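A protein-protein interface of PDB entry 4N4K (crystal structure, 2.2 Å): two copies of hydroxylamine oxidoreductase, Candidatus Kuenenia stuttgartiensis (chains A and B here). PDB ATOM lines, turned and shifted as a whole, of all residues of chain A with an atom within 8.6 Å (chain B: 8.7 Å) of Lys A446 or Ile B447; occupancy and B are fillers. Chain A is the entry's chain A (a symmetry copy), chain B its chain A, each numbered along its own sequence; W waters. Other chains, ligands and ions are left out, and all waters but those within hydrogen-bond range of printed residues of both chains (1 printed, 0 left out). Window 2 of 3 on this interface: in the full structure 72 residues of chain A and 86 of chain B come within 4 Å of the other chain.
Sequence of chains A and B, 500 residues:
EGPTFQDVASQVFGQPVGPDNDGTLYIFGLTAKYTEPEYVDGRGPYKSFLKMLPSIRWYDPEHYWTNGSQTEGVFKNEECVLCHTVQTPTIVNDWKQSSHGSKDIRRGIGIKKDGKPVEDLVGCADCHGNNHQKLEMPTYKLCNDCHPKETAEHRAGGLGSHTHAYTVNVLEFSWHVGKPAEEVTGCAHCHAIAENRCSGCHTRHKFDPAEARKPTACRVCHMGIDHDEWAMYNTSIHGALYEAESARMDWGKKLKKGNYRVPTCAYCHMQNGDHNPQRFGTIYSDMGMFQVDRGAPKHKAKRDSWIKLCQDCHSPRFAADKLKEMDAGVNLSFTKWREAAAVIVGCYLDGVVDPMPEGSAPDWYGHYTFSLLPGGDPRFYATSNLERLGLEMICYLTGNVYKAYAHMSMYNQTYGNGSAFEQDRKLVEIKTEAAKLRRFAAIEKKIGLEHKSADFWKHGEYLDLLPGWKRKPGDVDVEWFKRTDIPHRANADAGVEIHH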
ATOM      1  N   ARG A 439      17.594  16.881 -37.250  1.00  0.00           N
ATOM      2  CA  ARG A 439      18.421  16.703 -36.057  1.00  0.00           C
ATOM      3  C   ARG A 439      18.487  17.975 -35.209  1.00  0.00           C
ATOM      4  O   ARG A 439      18.525  17.891 -33.981  1.00  0.00           O
ATOM      5  CB  ARG A 439      19.830  16.226 -36.423  1.00  0.00           C
ATOM      6  CG  ARG A 439      19.870  14.774 -36.882  1.00  0.00           C
ATOM      7  CD  ARG A 439      21.256  14.361 -37.368  1.00  0.00           C
ATOM      8  NE  ARG A 439      22.115  13.868 -36.294  1.00  0.00           N
ATOM      9  CZ  ARG A 439      23.320  13.331 -36.478  1.00  0.00           C
ATOM     10  NH1 ARG A 439      23.954  13.478 -37.638  1.00  0.00           N
ATOM     11  NH2 ARG A 439      23.980  12.825 -35.442  1.00  0.00           N
ATOM     12  N   PHE A 440      18.518  19.141 -35.852  1.00  0.00           N
ATOM     13  CA  PHE A 440      18.484  20.410 -35.118  1.00  0.00           C
ATOM     14  C   PHE A 440      17.149  20.596 -34.396  1.00  0.00           C
ATOM     15  O   PHE A 440      17.121  21.027 -33.245  1.00  0.00           O
ATOM     16  CB  PHE A 440      18.734  21.614 -36.036  1.00  0.00           C
ATOM     17  CG  PHE A 440      20.194  21.922 -36.270  1.00  0.00           C
ATOM     18  CD1 PHE A 440      21.020  22.234 -35.195  1.00  0.00           C
ATOM     19  CD2 PHE A 440      20.643  22.226 -37.553  1.00  0.00           C
ATOM     20  CE1 PHE A 440      22.323  22.669 -35.399  1.00  0.00           C
ATOM     21  CE2 PHE A 440      21.945  22.675 -37.769  1.00  0.00           C
ATOM     22  CZ  PHE A 440      22.779  22.919 -36.686  1.00  0.00           C
ATOM     23  N   ALA A 441      16.052  20.276 -35.079  1.00  0.00           N
ATOM     24  CA  ALA A 441      14.712  20.412 -34.507  1.00  0.00           C
ATOM     25  C   ALA A 441      14.477  19.443 -33.342  1.00  0.00           C
ATOM     26  O   ALA A 441      13.938  19.837 -32.309  1.00  0.00           O
ATOM     27  CB  ALA A 441      13.653  20.211 -35.579  1.00  0.00           C
ATOM     28  N   ALA A 442      14.965  18.212 -33.480  1.00  0.00           N
ATOM     29  CA  ALA A 442      14.826  17.192 -32.433  1.00  0.00           C
ATOM     30  C   ALA A 442      15.646  17.532 -31.178  1.00  0.00           C
ATOM     31  O   ALA A 442      15.200  17.280 -30.055  1.00  0.00           O
ATOM     32  CB  ALA A 442      15.220  15.821 -32.969  1.00  0.00           C
ATOM     33  N   ILE A 443      16.838  18.093 -31.373  1.00  0.00           N
ATOM     34  CA  ILE A 443      17.665  18.568 -30.260  1.00  0.00           C
ATOM     35  C   ILE A 443      17.022  19.774 -29.568  1.00  0.00           C
ATOM     36  O   ILE A 443      16.824  19.767 -28.351  1.00  0.00           O
ATOM     37  CB  ILE A 443      19.092  18.940 -30.731  1.00  0.00           C
ATOM     38  CG1 ILE A 443      19.892  17.669 -31.030  1.00  0.00           C
ATOM     39  CG2 ILE A 443      19.815  19.766 -29.681  1.00  0.00           C
ATOM     40  CD1 ILE A 443      21.178  17.912 -31.791  1.00  0.00           C
ATOM     41  N   GLU A 444      16.656  20.781 -30.356  1.00  0.00           N
ATOM     42  CA  GLU A 444      16.037  22.001 -29.830  1.00  0.00           C
ATOM     43  C   GLU A 444      14.743  21.731 -29.055  1.00  0.00           C
ATOM     44  O   GLU A 444      14.462  22.396 -28.058  1.00  0.00           O
ATOM     45  CB  GLU A 444      15.778  22.997 -30.966  1.00  0.00           C
ATOM     46  CG  GLU A 444      17.032  23.742 -31.409  1.00  0.00           C
ATOM     47  CD  GLU A 444      16.923  24.348 -32.802  1.00  0.00           C
ATOM     48  OE1 GLU A 444      17.951  24.864 -33.295  1.00  0.00           O
ATOM     49  OE2 GLU A 444      15.819  24.328 -33.396  1.00  0.00           O
ATOM     50  N   LYS A 445      13.961  20.761 -29.518  1.00  0.00           N
ATOM     51  CA  LYS A 445      12.746  20.356 -28.816  1.00  0.00           C
ATOM     52  C   LYS A 445      13.068  19.744 -27.448  1.00  0.00           C
ATOM     53  O   LYS A 445      12.600  20.244 -26.422  1.00  0.00           O
ATOM     54  CB  LYS A 445      11.938  19.364 -29.660  1.00  0.00           C
ATOM     55  CG  LYS A 445      10.730  18.781 -28.938  1.00  0.00           C
ATOM     56  CD  LYS A 445       9.748  18.129 -29.895  1.00  0.00           C
ATOM     57  CE  LYS A 445       8.591  17.493 -29.131  1.00  0.00           C
ATOM     58  NZ  LYS A 445       7.674  16.741 -30.031  1.00  0.00           N
ATOM     59  N   LYS A 446      14.019  18.812 -27.427  1.00  0.00           N
ATOM     60  CA  LYS A 446      14.357  18.081 -26.205  1.00  0.00           C
ATOM     61  C   LYS A 446      14.919  18.978 -25.098  1.00  0.00           C
ATOM     62  O   LYS A 446      14.673  18.721 -23.920  1.00  0.00           O
ATOM     63  CB  LYS A 446      15.342  16.941 -26.492  1.00  0.00           C
ATOM     64  CG  LYS A 446      15.533  15.998 -25.307  1.00  0.00           C
ATOM     65  CD  LYS A 446      16.495  14.871 -25.609  1.00  0.00           C
ATOM     66  CE  LYS A 446      16.872  14.117 -24.330  1.00  0.00           C
ATOM     67  NZ  LYS A 446      15.696  13.511 -23.648  1.00  0.00           N
ATOM     68  N   ILE A 447      15.727  19.969 -25.468  1.00  0.00           N
ATOM     69  CA  ILE A 447      16.332  20.876 -24.485  1.00  0.00           C
ATOM     70  C   ILE A 447      15.518  22.159 -24.270  1.00  0.00           C
ATOM     71  O   ILE A 447      15.899  23.010 -23.466  1.00  0.00           O
ATOM     72  CB  ILE A 447      17.796  21.232 -24.857  1.00  0.00           C
ATOM     73  CG1 ILE A 447      17.855  22.220 -26.035  1.00  0.00           C
ATOM     74  CG2 ILE A 447      18.582  19.962 -25.170  1.00  0.00           C
ATOM     75  CD1 ILE A 447      19.270  22.544 -26.486  1.00  0.00           C
ATOM     76  N   GLY A 448      14.414  22.302 -25.001  1.00  0.00           N
ATOM     77  CA  GLY A 448      13.530  23.451 -24.847  1.00  0.00           C
ATOM     78  C   GLY A 448      14.112  24.766 -25.341  1.00  0.00           C
ATOM     79  O   GLY A 448      13.813  25.822 -24.781  1.00  0.00           O
ATOM     80  N   LEU A 449      14.946  24.706 -26.378  1.00  0.00           N
ATOM     81  CA  LEU A 449      15.462  25.913 -27.024  1.00  0.00           C
ATOM     82  C   LEU A 449      14.448  26.386 -28.069  1.00  0.00           C
ATOM     83  O   LEU A 449      13.995  25.592 -28.892  1.00  0.00           O
ATOM     84  CB  LEU A 449      16.818  25.631 -27.686  1.00  0.00           C
ATOM     85  CG  LEU A 449      17.743  26.830 -27.944  1.00  0.00           C
ATOM     86  CD1 LEU A 449      19.115  26.354 -28.392  1.00  0.00           C
ATOM     87  CD2 LEU A 449      17.159  27.792 -28.970  1.00  0.00           C
ATOM     88  N   PHE B 440      26.874  17.093 -34.047  1.00  0.00           N
ATOM     89  CA  PHE B 440      25.561  16.502 -33.771  1.00  0.00           C
ATOM     90  C   PHE B 440      25.679  15.309 -32.821  1.00  0.00           C
ATOM     91  O   PHE B 440      24.876  15.166 -31.902  1.00  0.00           O
ATOM     92  CB  PHE B 440      24.849  16.055 -35.056  1.00  0.00           C
ATOM     93  CG  PHE B 440      24.079  17.152 -35.751  1.00  0.00           C
ATOM     94  CD1 PHE B 440      23.043  17.803 -35.088  1.00  0.00           C
ATOM     95  CD2 PHE B 440      24.162  17.290 -37.134  1.00  0.00           C
ATOM     96  CE1 PHE B 440      22.224  18.704 -35.755  1.00  0.00           C
ATOM     97  CE2 PHE B 440      23.337  18.183 -37.816  1.00  0.00           C
ATOM     98  CZ  PHE B 440      22.351  18.874 -37.127  1.00  0.00           C
ATOM     99  N   ALA B 441      26.678  14.460 -33.053  1.00  0.00           N
ATOM    100  CA  ALA B 441      26.900  13.276 -32.222  1.00  0.00           C
ATOM    101  C   ALA B 441      27.314  13.640 -30.791  1.00  0.00           C
ATOM    102  O   ALA B 441      26.804  13.062 -29.832  1.00  0.00           O
ATOM    103  CB  ALA B 441      27.943  12.369 -32.856  1.00  0.00           C
ATOM    104  N   ALA B 442      28.164  14.656 -30.654  1.00  0.00           N
ATOM    105  CA  ALA B 442      28.628  15.119 -29.340  1.00  0.00           C
ATOM    106  C   ALA B 442      27.499  15.765 -28.521  1.00  0.00           C
ATOM    107  O   ALA B 442      27.437  15.591 -27.300  1.00  0.00           O
ATOM    108  CB  ALA B 442      29.791  16.090 -29.498  1.00  0.00           C
ATOM    109  N   ILE B 443      26.620  16.509 -29.191  1.00  0.00           N
ATOM    110  CA  ILE B 443      25.436  17.084 -28.546  1.00  0.00           C
ATOM    111  C   ILE B 443      24.448  15.990 -28.128  1.00  0.00           C
ATOM    112  O   ILE B 443      24.044  15.920 -26.966  1.00  0.00           O
ATOM    113  CB  ILE B 443      24.724  18.103 -29.468  1.00  0.00           C
ATOM    114  CG1 ILE B 443      25.540  19.395 -29.549  1.00  0.00           C
ATOM    115  CG2 ILE B 443      23.325  18.409 -28.965  1.00  0.00           C
ATOM    116  CD1 ILE B 443      25.109  20.331 -30.658  1.00  0.00           C
ATOM    117  N   GLU B 444      24.103  15.116 -29.069  1.00  0.00           N
ATOM    118  CA  GLU B 444      23.160  14.022 -28.814  1.00  0.00           C
ATOM    119  C   GLU B 444      23.611  13.094 -27.681  1.00  0.00           C
ATOM    120  O   GLU B 444      22.786  12.604 -26.910  1.00  0.00           O
ATOM    121  CB  GLU B 444      22.920  13.218 -30.097  1.00  0.00           C
ATOM    122  CG  GLU B 444      21.966  13.906 -31.067  1.00  0.00           C
ATOM    123  CD  GLU B 444      22.084  13.403 -32.499  1.00  0.00           C
ATOM    124  OE1 GLU B 444      21.432  14.003 -33.383  1.00  0.00           O
ATOM    125  OE2 GLU B 444      22.805  12.406 -32.743  1.00  0.00           O
ATOM    126  N   LYS B 445      24.915  12.854 -27.589  1.00  0.00           N
ATOM    127  CA  LYS B 445      25.471  12.053 -26.501  1.00  0.00           C
ATOM    128  C   LYS B 445      25.280  12.743 -25.146  1.00  0.00           C
ATOM    129  O   LYS B 445      24.655  12.174 -24.246  1.00  0.00           O
ATOM    130  CB  LYS B 445      26.959  11.771 -26.743  1.00  0.00           C
ATOM    131  CG  LYS B 445      27.648  11.066 -25.581  1.00  0.00           C
ATOM    132  CD  LYS B 445      28.978  10.456 -25.988  1.00  0.00           C
ATOM    133  CE  LYS B 445      29.672   9.825 -24.786  1.00  0.00           C
ATOM    134  NZ  LYS B 445      31.033   9.325 -25.125  1.00  0.00           N
ATOM    135  N   LYS B 446      25.627  14.027 -25.082  1.00  0.00           N
ATOM    136  CA  LYS B 446      25.584  14.776 -23.825  1.00  0.00           C
ATOM    137  C   LYS B 446      24.172  14.914 -23.249  1.00  0.00           C
ATOM    138  O   LYS B 446      24.007  14.921 -22.029  1.00  0.00           O
ATOM    139  CB  LYS B 446      26.211  16.167 -23.985  1.00  0.00           C
ATOM    140  CG  LYS B 446      26.416  16.890 -22.656  1.00  0.00           C
ATOM    141  CD  LYS B 446      27.049  18.254 -22.827  1.00  0.00           C
ATOM    142  CE  LYS B 446      26.986  19.053 -21.522  1.00  0.00           C
ATOM    143  NZ  LYS B 446      27.697  18.384 -20.399  1.00  0.00           N
ATOM    144  N   ILE B 447      23.176  15.100 -24.113  1.00  0.00           N
ATOM    145  CA  ILE B 447      21.787  15.260 -23.665  1.00  0.00           C
ATOM    146  C   ILE B 447      21.002  13.941 -23.662  1.00  0.00           C
ATOM    147  O   ILE B 447      19.825  13.919 -23.300  1.00  0.00           O
ATOM    148  CB  ILE B 447      21.033  16.325 -24.503  1.00  0.00           C
ATOM    149  CG1 ILE B 447      20.682  15.798 -25.905  1.00  0.00           C
ATOM    150  CG2 ILE B 447      21.860  17.605 -24.592  1.00  0.00           C
ATOM    151  CD1 ILE B 447      20.006  16.832 -26.791  1.00  0.00           C
ATOM    152  N   GLY B 448      21.646  12.855 -24.082  1.00  0.00           N
ATOM    153  CA  GLY B 448      21.023  11.537 -24.074  1.00  0.00           C
ATOM    154  C   GLY B 448      19.910  11.357 -25.095  1.00  0.00           C
ATOM    155  O   GLY B 448      18.952  10.626 -24.841  1.00  0.00           O
ATOM    156  N   LEU B 449      20.027  12.027 -26.240  1.00  0.00           N
ATOM    157  CA  LEU B 449      19.092  11.832 -27.347  1.00  0.00           C
ATOM    158  C   LEU B 449      19.557  10.636 -28.182  1.00  0.00           C
ATOM    159  O   LEU B 449      20.725  10.566 -28.560  1.00  0.00           O
ATOM    160  CB  LEU B 449      19.017  13.094 -28.218  1.00  0.00           C
ATOM    161  CG  LEU B 449      17.758  13.288 -29.077  1.00  0.00           C
ATOM    162  CD1 LEU B 449      17.749  14.677 -29.696  1.00  0.00           C
ATOM    163  CD2 LEU B 449      17.639  12.228 -30.163  1.00  0.00           C
ATOM    164  N   GLU B 450      18.684   9.643 -28.341  1.00  0.00           N
ATOM    165  CA  GLU B 450      18.994   8.453 -29.143  1.00  0.00           C
ATOM    166  C   GLU B 450      18.632   8.705 -30.605  1.00  0.00           C
ATOM    167  O   GLU B 450      17.466   8.598 -30.991  1.00  0.00           O
ATOM    168  CB  GLU B 450      18.237   7.221 -28.621  1.00  0.00           C
ATOM    169  CG  GLU B 450      18.625   6.772 -27.204  1.00  0.00           C
ATOM    170  CD  GLU B 450      20.108   6.417 -27.057  1.00  0.00           C
ATOM    171  OE1 GLU B 450      20.759   6.959 -26.130  1.00  0.00           O
ATOM    172  OE2 GLU B 450      20.635   5.643 -27.892  1.00  0.00           O
HETATM  173  O   HOH W   1      19.062  14.941 -33.061  1.00  0.00           O
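The guanidinium group (NH2) of Arg A439 lies within salt-bridge range of the side-chain carboxylate (OE2) of Glu B444 (3.0 Å).
The backbone carbonyl oxygen (O) of Glu B444 is in hydrogen-bond range of the backbone NH (N) of Leu B449, 2.9 Å away.
Among the printed residues, merely in contact across the chains: Lys A446 with Ile B447 (3.1 Å), Arg A439 with Phe B440 (3.4 Å), Ile A443 with Ile B443 (3.6 Å), Ala A442 with Leu B449 (3.7 Å), Phe A440 with Phe B440 (3.7 Å), Ile A443 with Phe B440 (3.8 Å), Ile A447 with Ile B447 (3.8 Å), Ile A443 with Leu B449 (3.9 Å) and Arg A439 with Ala B441 (3.96 Å).
Printed residues of chain B within 4 Å of Lys A446: Ile B447 (3.1 Å). Of chain A, only Lys A446 (3.1 Å) and Ile A447 (3.8 Å) come within 4 Å of Ile B447. No residue of chain A comes within 4 Å of Gly B448. Of the printed residues of chain B, Phe A440 touches Phe B440 (3.7 Å). Printed residues of chain A within 4 Å of Phe B440: Arg A439, Phe A440 and Ile A443. Printed residues of chain A within 4 Å of Ile B443: Ile A443 (3.6 Å). Printed residues of chain A within 4 Å of Ala B441: Arg A439 (3.96 Å). Of the printed residues of chain B, Arg A439 touches Phe B440, Ala B441 and Glu B444. Ala A441 touches none of the printed residues of chain B. The nearest printed residue of chain B that does not touch Lys A446 is Leu B449 (4.02 Å). The nearest residue of chain A that does not touch Ile B447 is Ile A443 (4.1 Å). The nearest printed residue of chain B that does not touch Ile A443 is Ile B447 (4.1 Å).
Hydrophobic or aromatic side chains of chain B that line the printed part of chain A: Phe B440, Ile B443, Ile B447 and Leu B449. Of the 11 printed residues of chain A, 6 touch a printed residue of chain B. Among the printed residues, 10 pairs touch across the chains. Among the printed residues, Asp or Glu carboxylates within 4 Å of a Lys or Arg side-chain nitrogen of the other chain: Arg A439 with Glu B444.
Phe A440 touches its own counterpart, Phe B440. Ile A443 touches Phe B440, but with the chains exchanged Phe A440 does not touch Ile B443 (6.0 Å). Ile A443 touches Leu B449, but with the chains exchanged Leu A449 does not touch Ile B443 (8.8 Å). Ile B447 touches its own counterpart, Ile A447. Positions printed for both chains: 440, 441, 442, 443, 444, 445, 446, 447, 448 and 449. Of the 10 pairs that touch across the chains among the printed residues, 3 have their exchanged pair printed and touching as well.
Water W1 bridges the side-chain carboxylate of Glu B444 (2.6 Å) and the backbone carbonyl oxygen of Arg A439 (3.1 Å).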
